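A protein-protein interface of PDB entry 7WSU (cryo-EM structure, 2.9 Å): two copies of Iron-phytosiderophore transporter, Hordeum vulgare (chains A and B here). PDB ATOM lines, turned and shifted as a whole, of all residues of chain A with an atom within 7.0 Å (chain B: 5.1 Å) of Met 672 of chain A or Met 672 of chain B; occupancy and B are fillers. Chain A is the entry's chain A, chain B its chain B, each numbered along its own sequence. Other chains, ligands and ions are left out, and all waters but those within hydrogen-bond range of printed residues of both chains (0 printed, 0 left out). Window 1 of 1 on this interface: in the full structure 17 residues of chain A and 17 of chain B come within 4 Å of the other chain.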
ATOM      1  N   PHE A 240      22.980 -32.179 -27.484  1.00  0.00           N
ATOM      2  CA  PHE A 240      21.525 -32.105 -27.586  1.00  0.00           C
ATOM      3  C   PHE A 240      20.916 -31.426 -26.365  1.00  0.00           C
ATOM      4  O   PHE A 240      19.934 -30.685 -26.485  1.00  0.00           O
ATOM      5  CB  PHE A 240      20.950 -33.509 -27.771  1.00  0.00           C
ATOM      6  CG  PHE A 240      19.450 -33.548 -27.867  1.00  0.00           C
ATOM      7  CD1 PHE A 240      18.808 -33.154 -29.027  1.00  0.00           C
ATOM      8  CD2 PHE A 240      18.686 -33.986 -26.800  1.00  0.00           C
ATOM      9  CE1 PHE A 240      17.431 -33.190 -29.119  1.00  0.00           C
ATOM     10  CE2 PHE A 240      17.308 -34.024 -26.886  1.00  0.00           C
ATOM     11  CZ  PHE A 240      16.682 -33.626 -28.047  1.00  0.00           C
ATOM     12  N   GLN A 241      21.484 -31.669 -25.180  1.00  0.00           N
ATOM     13  CA  GLN A 241      20.936 -31.097 -23.953  1.00  0.00           C
ATOM     14  C   GLN A 241      21.047 -29.580 -23.928  1.00  0.00           C
ATOM     15  O   GLN A 241      20.246 -28.912 -23.263  1.00  0.00           O
ATOM     16  CB  GLN A 241      21.659 -31.671 -22.737  1.00  0.00           C
ATOM     17  CG  GLN A 241      21.322 -33.103 -22.399  1.00  0.00           C
ATOM     18  CD  GLN A 241      21.956 -33.537 -21.099  1.00  0.00           C
ATOM     19  OE1 GLN A 241      21.468 -33.217 -20.017  1.00  0.00           O
ATOM     20  NE2 GLN A 241      23.067 -34.256 -21.195  1.00  0.00           N
ATOM     21  N   PHE A 243      20.471 -27.134 -26.019  1.00  0.00           N
ATOM     22  CA  PHE A 243      19.428 -26.309 -26.610  1.00  0.00           C
ATOM     23  C   PHE A 243      18.215 -26.131 -25.707  1.00  0.00           C
ATOM     24  O   PHE A 243      17.383 -25.263 -25.990  1.00  0.00           O
ATOM     25  CB  PHE A 243      18.985 -26.911 -27.942  1.00  0.00           C
ATOM     26  CG  PHE A 243      20.048 -26.886 -28.998  1.00  0.00           C
ATOM     27  CD1 PHE A 243      20.265 -25.747 -29.751  1.00  0.00           C
ATOM     28  CD2 PHE A 243      20.831 -27.999 -29.232  1.00  0.00           C
ATOM     29  CE1 PHE A 243      21.244 -25.723 -30.722  1.00  0.00           C
ATOM     30  CE2 PHE A 243      21.810 -27.977 -30.202  1.00  0.00           C
ATOM     31  CZ  PHE A 243      22.016 -26.838 -30.947  1.00  0.00           C
ATOM     32  N   TYR A 244      18.092 -26.916 -24.641  1.00  0.00           N
ATOM     33  CA  TYR A 244      16.905 -26.887 -23.800  1.00  0.00           C
ATOM     34  C   TYR A 244      17.174 -26.398 -22.384  1.00  0.00           C
ATOM     35  O   TYR A 244      16.232 -26.306 -21.591  1.00  0.00           O
ATOM     36  CB  TYR A 244      16.262 -28.279 -23.761  1.00  0.00           C
ATOM     37  CG  TYR A 244      15.976 -28.815 -25.143  1.00  0.00           C
ATOM     38  CD1 TYR A 244      14.834 -28.430 -25.834  1.00  0.00           C
ATOM     39  CD2 TYR A 244      16.856 -29.684 -25.771  1.00  0.00           C
ATOM     40  CE1 TYR A 244      14.573 -28.907 -27.101  1.00  0.00           C
ATOM     41  CE2 TYR A 244      16.603 -30.164 -27.037  1.00  0.00           C
ATOM     42  CZ  TYR A 244      15.461 -29.772 -27.697  1.00  0.00           C
ATOM     43  OH  TYR A 244      15.204 -30.250 -28.959  1.00  0.00           O
ATOM     44  N   THR A 245      18.421 -26.086 -22.045  1.00  0.00           N
ATOM     45  CA  THR A 245      18.752 -25.470 -20.760  1.00  0.00           C
ATOM     46  C   THR A 245      18.800 -23.950 -20.877  1.00  0.00           C
ATOM     47  O   THR A 245      19.785 -23.310 -20.521  1.00  0.00           O
ATOM     48  CB  THR A 245      20.074 -26.019 -20.244  1.00  0.00           C
ATOM     49  OG1 THR A 245      21.101 -25.786 -21.217  1.00  0.00           O
ATOM     50  CG2 THR A 245      19.966 -27.509 -19.983  1.00  0.00           C
ATOM     51  N   GLY A 246      17.719 -23.360 -21.382  1.00  0.00           N
ATOM     52  CA  GLY A 246      17.689 -21.935 -21.642  1.00  0.00           C
ATOM     53  C   GLY A 246      16.947 -21.131 -20.599  1.00  0.00           C
ATOM     54  O   GLY A 246      16.216 -20.195 -20.932  1.00  0.00           O
ATOM     55  N   GLY A 247      17.126 -21.481 -19.332  1.00  0.00           N
ATOM     56  CA  GLY A 247      16.468 -20.756 -18.263  1.00  0.00           C
ATOM     57  C   GLY A 247      16.980 -21.211 -16.917  1.00  0.00           C
ATOM     58  O   GLY A 247      17.780 -22.145 -16.813  1.00  0.00           O
ATOM     59  N   ALA A 249      16.936 -23.176 -13.785  1.00  0.00           N
ATOM     60  CA  ALA A 249      16.405 -24.455 -13.315  1.00  0.00           C
ATOM     61  C   ALA A 249      15.386 -25.031 -14.303  1.00  0.00           C
ATOM     62  O   ALA A 249      14.218 -25.252 -13.981  1.00  0.00           O
ATOM     63  CB  ALA A 249      15.801 -24.317 -11.912  1.00  0.00           C
ATOM     64  N   CYS A 250      15.857 -25.270 -15.524  1.00  0.00           N
ATOM     65  CA  CYS A 250      15.036 -25.904 -16.543  1.00  0.00           C
ATOM     66  C   CYS A 250      15.948 -26.582 -17.555  1.00  0.00           C
ATOM     67  O   CYS A 250      17.009 -26.052 -17.894  1.00  0.00           O
ATOM     68  CB  CYS A 250      14.108 -24.895 -17.233  1.00  0.00           C
ATOM     69  SG  CYS A 250      14.818 -23.950 -18.596  1.00  0.00           S
ATOM     70  N   GLY A 251      15.533 -27.757 -18.019  1.00  0.00           N
ATOM     71  CA  GLY A 251      16.338 -28.550 -18.928  1.00  0.00           C
ATOM     72  C   GLY A 251      16.456 -29.986 -18.464  1.00  0.00           C
ATOM     73  O   GLY A 251      15.830 -30.372 -17.473  1.00  0.00           O
ATOM     74  N   PHE A 252      17.251 -30.791 -19.171  1.00  0.00           N
ATOM     75  CA  PHE A 252      17.455 -32.174 -18.754  1.00  0.00           C
ATOM     76  C   PHE A 252      18.244 -32.276 -17.456  1.00  0.00           C
ATOM     77  O   PHE A 252      18.116 -33.279 -16.747  1.00  0.00           O
ATOM     78  CB  PHE A 252      18.167 -32.964 -19.853  1.00  0.00           C
ATOM     79  CG  PHE A 252      17.235 -33.704 -20.767  1.00  0.00           C
ATOM     80  CD1 PHE A 252      16.493 -34.773 -20.299  1.00  0.00           C
ATOM     81  CD2 PHE A 252      17.104 -33.332 -22.093  1.00  0.00           C
ATOM     82  CE1 PHE A 252      15.635 -35.459 -21.137  1.00  0.00           C
ATOM     83  CE2 PHE A 252      16.247 -34.013 -22.936  1.00  0.00           C
ATOM     84  CZ  PHE A 252      15.513 -35.077 -22.456  1.00  0.00           C
ATOM     85  N   VAL A 253      19.058 -31.270 -17.137  1.00  0.00           N
ATOM     86  CA  VAL A 253      19.819 -31.304 -15.892  1.00  0.00           C
ATOM     87  C   VAL A 253      18.889 -31.155 -14.691  1.00  0.00           C
ATOM     88  O   VAL A 253      19.088 -31.799 -13.656  1.00  0.00           O
ATOM     89  CB  VAL A 253      20.924 -30.229 -15.914  1.00  0.00           C
ATOM     90  CG1 VAL A 253      20.334 -28.833 -16.070  1.00  0.00           C
ATOM     91  CG2 VAL A 253      21.776 -30.317 -14.658  1.00  0.00           C
ATOM     92  N   GLN A 254      17.870 -30.309 -14.802  1.00  0.00           N
ATOM     93  CA  GLN A 254      16.881 -30.138 -13.736  1.00  0.00           C
ATOM     94  C   GLN A 254      15.634 -30.975 -14.017  1.00  0.00           C
ATOM     95  O   GLN A 254      14.519 -30.467 -14.110  1.00  0.00           O
ATOM     96  CB  GLN A 254      16.537 -28.661 -13.577  1.00  0.00           C
ATOM     97  CG  GLN A 254      17.731 -27.781 -13.258  1.00  0.00           C
ATOM     98  CD  GLN A 254      18.352 -28.102 -11.916  1.00  0.00           C
ATOM     99  OE1 GLN A 254      17.721 -27.940 -10.872  1.00  0.00           O
ATOM    100  NE2 GLN A 254      19.601 -28.551 -11.935  1.00  0.00           N
ATOM    101  N   PHE A 255      15.834 -32.287 -14.143  1.00  0.00           N
ATOM    102  CA  PHE A 255      14.753 -33.194 -14.492  1.00  0.00           C
ATOM    103  C   PHE A 255      14.183 -33.832 -13.236  1.00  0.00           C
ATOM    104  O   PHE A 255      14.911 -34.556 -12.540  1.00  0.00           O
ATOM    105  CB  PHE A 255      15.244 -34.272 -15.453  1.00  0.00           C
ATOM    106  CG  PHE A 255      14.165 -34.847 -16.325  1.00  0.00           C
ATOM    107  CD1 PHE A 255      13.199 -35.688 -15.796  1.00  0.00           C
ATOM    108  CD2 PHE A 255      14.111 -34.543 -17.673  1.00  0.00           C
ATOM    109  CE1 PHE A 255      12.205 -36.213 -16.594  1.00  0.00           C
ATOM    110  CE2 PHE A 255      13.118 -35.069 -18.476  1.00  0.00           C
ATOM    111  CZ  PHE A 255      12.165 -35.904 -17.935  1.00  0.00           C
ATOM    112  N   ILE A 670      15.571 -22.717 -26.114  1.00  0.00           N
ATOM    113  CA  ILE A 670      14.398 -23.313 -25.486  1.00  0.00           C
ATOM    114  C   ILE A 670      14.699 -23.571 -24.016  1.00  0.00           C
ATOM    115  O   ILE A 670      15.842 -23.824 -23.629  1.00  0.00           O
ATOM    116  CB  ILE A 670      13.977 -24.618 -26.201  1.00  0.00           C
ATOM    117  CG1 ILE A 670      13.915 -24.401 -27.712  1.00  0.00           C
ATOM    118  CG2 ILE A 670      12.633 -25.107 -25.701  1.00  0.00           C
ATOM    119  CD1 ILE A 670      13.887 -25.679 -28.510  1.00  0.00           C
ATOM    120  N   CYS A 671      13.655 -23.491 -23.192  1.00  0.00           N
ATOM    121  CA  CYS A 671      13.739 -23.768 -21.764  1.00  0.00           C
ATOM    122  C   CYS A 671      12.702 -24.825 -21.411  1.00  0.00           C
ATOM    123  O   CYS A 671      11.498 -24.560 -21.474  1.00  0.00           O
ATOM    124  CB  CYS A 671      13.522 -22.493 -20.946  1.00  0.00           C
ATOM    125  SG  CYS A 671      13.291 -22.739 -19.171  1.00  0.00           S
ATOM    126  N   MET A 672      13.172 -26.015 -21.036  1.00  0.00           N
ATOM    127  CA  MET A 672      12.301 -27.145 -20.714  1.00  0.00           C
ATOM    128  C   MET A 672      11.902 -27.052 -19.248  1.00  0.00           C
ATOM    129  O   MET A 672      12.626 -27.490 -18.355  1.00  0.00           O
ATOM    130  CB  MET A 672      13.007 -28.462 -21.015  1.00  0.00           C
ATOM    131  CG  MET A 672      12.143 -29.695 -20.830  1.00  0.00           C
ATOM    132  SD  MET A 672      13.117 -31.172 -20.489  1.00  0.00           S
ATOM    133  CE  MET A 672      14.125 -31.262 -21.962  1.00  0.00           C
ATOM    134  N   LYS A 673      10.725 -26.488 -18.997  1.00  0.00           N
ATOM    135  CA  LYS A 673      10.222 -26.305 -17.642  1.00  0.00           C
ATOM    136  C   LYS A 673       9.328 -27.468 -17.240  1.00  0.00           C
ATOM    137  O   LYS A 673       8.711 -28.118 -18.088  1.00  0.00           O
ATOM    138  CB  LYS A 673       9.441 -24.995 -17.513  1.00  0.00           C
ATOM    139  CG  LYS A 673      10.296 -23.753 -17.602  1.00  0.00           C
ATOM    140  CD  LYS A 673       9.451 -22.500 -17.473  1.00  0.00           C
ATOM    141  CE  LYS A 673       8.942 -22.334 -16.052  1.00  0.00           C
ATOM    142  NZ  LYS A 673      10.051 -22.062 -15.094  1.00  0.00           N
ATOM    143  N   PHE A 674       9.270 -27.727 -15.935  1.00  0.00           N
ATOM    144  CA  PHE A 674       8.398 -28.742 -15.360  1.00  0.00           C
ATOM    145  C   PHE A 674       7.473 -28.063 -14.364  1.00  0.00           C
ATOM    146  O   PHE A 674       7.936 -27.336 -13.478  1.00  0.00           O
ATOM    147  CB  PHE A 674       9.211 -29.847 -14.684  1.00  0.00           C
ATOM    148  CG  PHE A 674      10.122 -30.586 -15.620  1.00  0.00           C
ATOM    149  CD1 PHE A 674      11.361 -30.067 -15.956  1.00  0.00           C
ATOM    150  CD2 PHE A 674       9.742 -31.798 -16.163  1.00  0.00           C
ATOM    151  CE1 PHE A 674      12.199 -30.743 -16.814  1.00  0.00           C
ATOM    152  CE2 PHE A 674      10.577 -32.478 -17.021  1.00  0.00           C
ATOM    153  CZ  PHE A 674      11.808 -31.948 -17.347  1.00  0.00           C
ATOM    154  N   LEU A 675       6.172 -28.299 -14.507  1.00  0.00           N
ATOM    155  CA  LEU A 675       5.175 -27.648 -13.677  1.00  0.00           C
ATOM    156  C   LEU A 675       4.224 -28.681 -13.085  1.00  0.00           C
ATOM    157  O   LEU A 675       4.021 -29.747 -13.673  1.00  0.00           O
ATOM    158  CB  LEU A 675       4.380 -26.616 -14.489  1.00  0.00           C
ATOM    159  CG  LEU A 675       5.186 -25.419 -14.992  1.00  0.00           C
ATOM    160  CD1 LEU A 675       4.337 -24.540 -15.891  1.00  0.00           C
ATOM    161  CD2 LEU A 675       5.747 -24.617 -13.830  1.00  0.00           C
ATOM    162  N   TYR B 244       4.562 -37.191 -17.088  1.00  0.00           N
ATOM    163  CA  TYR B 244       4.943 -35.853 -17.515  1.00  0.00           C
ATOM    164  C   TYR B 244       4.051 -35.289 -18.613  1.00  0.00           C
ATOM    165  O   TYR B 244       4.265 -34.148 -19.032  1.00  0.00           O
ATOM    166  CB  TYR B 244       6.406 -35.851 -17.974  1.00  0.00           C
ATOM    167  CG  TYR B 244       7.336 -36.405 -16.922  1.00  0.00           C
ATOM    168  CD1 TYR B 244       7.781 -35.610 -15.874  1.00  0.00           C
ATOM    169  CD2 TYR B 244       7.750 -37.729 -16.958  1.00  0.00           C
ATOM    170  CE1 TYR B 244       8.620 -36.113 -14.903  1.00  0.00           C
ATOM    171  CE2 TYR B 244       8.588 -38.239 -15.992  1.00  0.00           C
ATOM    172  CZ  TYR B 244       9.020 -37.428 -14.967  1.00  0.00           C
ATOM    173  OH  TYR B 244       9.857 -37.933 -14.003  1.00  0.00           O
ATOM    174  N   CYS B 250       2.103 -30.888 -23.799  1.00  0.00           N
ATOM    175  CA  CYS B 250       3.300 -30.890 -22.973  1.00  0.00           C
ATOM    176  C   CYS B 250       3.636 -32.326 -22.600  1.00  0.00           C
ATOM    177  O   CYS B 250       2.738 -33.132 -22.345  1.00  0.00           O
ATOM    178  CB  CYS B 250       3.121 -30.026 -21.716  1.00  0.00           C
ATOM    179  SG  CYS B 250       2.319 -30.814 -20.305  1.00  0.00           S
ATOM    180  N   GLY B 251       4.928 -32.637 -22.586  1.00  0.00           N
ATOM    181  CA  GLY B 251       5.390 -33.987 -22.326  1.00  0.00           C
ATOM    182  C   GLY B 251       6.391 -34.447 -23.363  1.00  0.00           C
ATOM    183  O   GLY B 251       6.785 -33.668 -24.235  1.00  0.00           O
ATOM    184  N   PHE B 252       6.817 -35.709 -23.281  1.00  0.00           N
ATOM    185  CA  PHE B 252       7.742 -36.239 -24.277  1.00  0.00           C
ATOM    186  C   PHE B 252       7.097 -36.380 -25.649  1.00  0.00           C
ATOM    187  O   PHE B 252       7.809 -36.367 -26.657  1.00  0.00           O
ATOM    188  CB  PHE B 252       8.296 -37.592 -23.826  1.00  0.00           C
ATOM    189  CG  PHE B 252       9.609 -37.499 -23.108  1.00  0.00           C
ATOM    190  CD1 PHE B 252      10.753 -37.109 -23.782  1.00  0.00           C
ATOM    191  CD2 PHE B 252       9.701 -37.804 -21.762  1.00  0.00           C
ATOM    192  CE1 PHE B 252      11.966 -37.024 -23.125  1.00  0.00           C
ATOM    193  CE2 PHE B 252      10.910 -37.720 -21.100  1.00  0.00           C
ATOM    194  CZ  PHE B 252      12.043 -37.329 -21.784  1.00  0.00           C
ATOM    195  N   PHE B 255       7.527 -33.016 -27.947  1.00  0.00           N
ATOM    196  CA  PHE B 255       8.915 -32.629 -27.755  1.00  0.00           C
ATOM    197  C   PHE B 255       9.420 -31.881 -28.978  1.00  0.00           C
ATOM    198  O   PHE B 255       9.465 -32.467 -30.071  1.00  0.00           O
ATOM    199  CB  PHE B 255       9.784 -33.854 -27.492  1.00  0.00           C
ATOM    200  CG  PHE B 255      11.029 -33.559 -26.704  1.00  0.00           C
ATOM    201  CD1 PHE B 255      12.085 -32.872 -27.279  1.00  0.00           C
ATOM    202  CD2 PHE B 255      11.142 -33.963 -25.386  1.00  0.00           C
ATOM    203  CE1 PHE B 255      13.226 -32.596 -26.557  1.00  0.00           C
ATOM    204  CE2 PHE B 255      12.284 -33.691 -24.660  1.00  0.00           C
ATOM    205  CZ  PHE B 255      13.326 -33.006 -25.246  1.00  0.00           C
ATOM    206  N   ILE B 670       2.785 -34.111 -13.411  1.00  0.00           N
ATOM    207  CA  ILE B 670       3.723 -33.118 -13.920  1.00  0.00           C
ATOM    208  C   ILE B 670       3.414 -32.847 -15.385  1.00  0.00           C
ATOM    209  O   ILE B 670       2.936 -33.720 -16.114  1.00  0.00           O
ATOM    210  CB  ILE B 670       5.187 -33.579 -13.739  1.00  0.00           C
ATOM    211  CG1 ILE B 670       5.417 -34.079 -12.314  1.00  0.00           C
ATOM    212  CG2 ILE B 670       6.158 -32.457 -14.048  1.00  0.00           C
ATOM    213  CD1 ILE B 670       6.677 -34.888 -12.147  1.00  0.00           C
ATOM    214  N   CYS B 671       3.683 -31.613 -15.812  1.00  0.00           N
ATOM    215  CA  CYS B 671       3.512 -31.190 -17.196  1.00  0.00           C
ATOM    216  C   CYS B 671       4.827 -30.602 -17.691  1.00  0.00           C
ATOM    217  O   CYS B 671       5.246 -29.538 -17.226  1.00  0.00           O
ATOM    218  CB  CYS B 671       2.375 -30.172 -17.321  1.00  0.00           C
ATOM    219  SG  CYS B 671       2.256 -29.333 -18.915  1.00  0.00           S
ATOM    220  N   MET B 672       5.467 -31.292 -18.635  1.00  0.00           N
ATOM    221  CA  MET B 672       6.763 -30.882 -19.175  1.00  0.00           C
ATOM    222  C   MET B 672       6.529 -29.902 -20.316  1.00  0.00           C
ATOM    223  O   MET B 672       6.292 -30.291 -21.460  1.00  0.00           O
ATOM    224  CB  MET B 672       7.553 -32.099 -19.640  1.00  0.00           C
ATOM    225  CG  MET B 672       8.964 -31.792 -20.106  1.00  0.00           C
ATOM    226  SD  MET B 672       9.588 -33.021 -21.266  1.00  0.00           S
ATOM    227  CE  MET B 672       9.508 -34.501 -20.268  1.00  0.00           C
ATOM    228  N   LYS B 673       6.611 -28.613 -20.006  1.00  0.00           N
ATOM    229  CA  LYS B 673       6.384 -27.559 -20.987  1.00  0.00           C
ATOM    230  C   LYS B 673       7.699 -27.109 -21.605  1.00  0.00           C
ATOM    231  O   LYS B 673       8.760 -27.213 -20.985  1.00  0.00           O
ATOM    232  CB  LYS B 673       5.681 -26.356 -20.356  1.00  0.00           C
ATOM    233  CG  LYS B 673       4.243 -26.612 -19.968  1.00  0.00           C
ATOM    234  CD  LYS B 673       3.619 -25.378 -19.345  1.00  0.00           C
ATOM    235  CE  LYS B 673       3.393 -24.298 -20.389  1.00  0.00           C
ATOM    236  NZ  LYS B 673       2.360 -24.700 -21.386  1.00  0.00           N
ATOM    237  N   PHE B 674       7.618 -26.614 -22.838  1.00  0.00           N
ATOM    238  CA  PHE B 674       8.757 -26.052 -23.550  1.00  0.00           C
ATOM    239  C   PHE B 674       8.430 -24.611 -23.905  1.00  0.00           C
ATOM    240  O   PHE B 674       7.375 -24.336 -24.488  1.00  0.00           O
ATOM    241  CB  PHE B 674       9.076 -26.864 -24.806  1.00  0.00           C
ATOM    242  CG  PHE B 674       9.444 -28.292 -24.526  1.00  0.00           C
ATOM    243  CD1 PHE B 674       8.462 -29.247 -24.322  1.00  0.00           C
ATOM    244  CD2 PHE B 674      10.769 -28.679 -24.467  1.00  0.00           C
ATOM    245  CE1 PHE B 674       8.798 -30.557 -24.065  1.00  0.00           C
ATOM    246  CE2 PHE B 674      11.109 -29.989 -24.211  1.00  0.00           C
ATOM    247  CZ  PHE B 674      10.120 -30.929 -24.009  1.00  0.00           C
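O of Tyr 244 of chain A is in hydrogen-bond range of N of Met 672 of chain A. The side-chain sulfur (SG) of Cys 250 of chain A forms a disulfide with the side-chain sulfur (SG) of Cys 671 of chain A, 2.0 Å away. SG of Cys 250 of chain A is in hydrogen-bond range of N of Met 672 of chain A (3.6 Å). The backbone carbonyl oxygen (O) of Tyr 244 of chain B sits at hydrogen-bond distance from the backbone NH (N) of Met 672 of chain B, at 3.1 Å. The side-chain sulfur (SG) of Cys 250 of chain B is disulfide-bonded to the side-chain sulfur (SG) of Cys 671 of chain B, at 2.0 Å. The backbone NH (N) of Met 672 of chain B lies within hydrogen-bond range of the side-chain sulfur (SG) of Cys 250 of chain B.
O of Lys 673 of chain A sits at hydrogen-bond distance from N of Lys 673 of chain B (2.9 Å). The backbone carbonyl oxygen (O) of Leu 675 of chain A sits at hydrogen-bond distance from the backbone NH (N) of Cys 671 of chain B (2.9 Å).
Of chain B, only Phe 255, Met 672, Lys 673 and Phe 674 come within 4 Å of Met 672 of chain A. Printed residues of chain B within 4 Å of Phe 674 of chain A: Cys 671 (3.7 Å) and Met 672 (3.5 Å). Printed residues of chain A within 4 Å of Phe 252 of chain B: Phe 255 (3.9 Å). Printed residues of chain B within 4 Å of Phe 255 of chain A: Tyr 244, Phe 252 and Met 672. Of the printed residues of chain B, Phe 252 of chain A touches Phe 255. Gly 247 of chain A touches none of the printed residues of chain B. The nearest printed residue of chain B that does not touch Met 672 of chain A is Phe 252 of chain B (6.3 Å). The nearest residue of chain A that does not touch Met 672 of chain B is Leu 675 of chain A (5.1 Å).
Among the printed residues, merely in contact across the chains: Phe 240 of chain A with Phe 255 of chain B (3.9 Å), Tyr 244 of chain A with Phe 255 of chain B (3.8 Å), Phe 252 of chain A with Phe 255 of chain B (3.9 Å), Phe 255 of chain A with Tyr 244 of chain B (3.8 Å), Phe 255 of chain A with Phe 252 of chain B (3.9 Å), Phe 255 of chain A with Met 672 of chain B (3.8 Å), Cys 671 of chain A with Lys 673 of chain B (3.8 Å), Cys 671 of chain A with Phe 674 of chain B (3.7 Å), Met 672 of chain A with Phe 255 of chain B (3.8 Å), Met 672 of chain A with Met 672 of chain B (3.9 Å), Met 672 of chain A with Lys 673 of chain B (3.6 Å), Met 672 of chain A with Phe 674 of chain B (3.5 Å), Lys 673 of chain A with Cys 671 of chain B (3.8 Å), Lys 673 of chain A with Met 672 of chain B (3.6 Å), Phe 674 of chain A with Cys 671 of chain B (3.7 Å), Phe 674 of chain A with Met 672 of chain B (3.5 Å), Leu 675 of chain A with Ile 670 of chain B (3.4 Å) and Leu 675 of chain A with Lys 673 of chain B (3.6 Å).
Tyr 244 of chain A touches Phe 255 of chain B, and with the chains exchanged Phe 255 of chain A touches Tyr 244 of chain B. Met 672 of chain B touches its own counterpart, Met 672 of chain A. Met 672 of chain A touches Lys 673 of chain B, and with the chains exchanged Lys 673 of chain A touches Met 672 of chain B. Lys 673 of chain A touches its own counterpart, Lys 673 of chain B. 10 positions are printed for both chains. Of the 20 pairs that touch across the chains among the printed residues, 16 have their exchanged pair printed and touching as well.
Of the 10 printed residues of chain B, 8 touch a printed residue of chain A. Printed residues of chain B that touch a printed residue of chain A: Tyr 244, Phe 252, Phe 255, Ile 670, Cys 671, Met 672, Lys 673 and Phe 674. Among the printed residues, no Asp or Glu carboxylate lies within 4 Å of a Lys or Arg side-chain nitrogen of the other chain.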
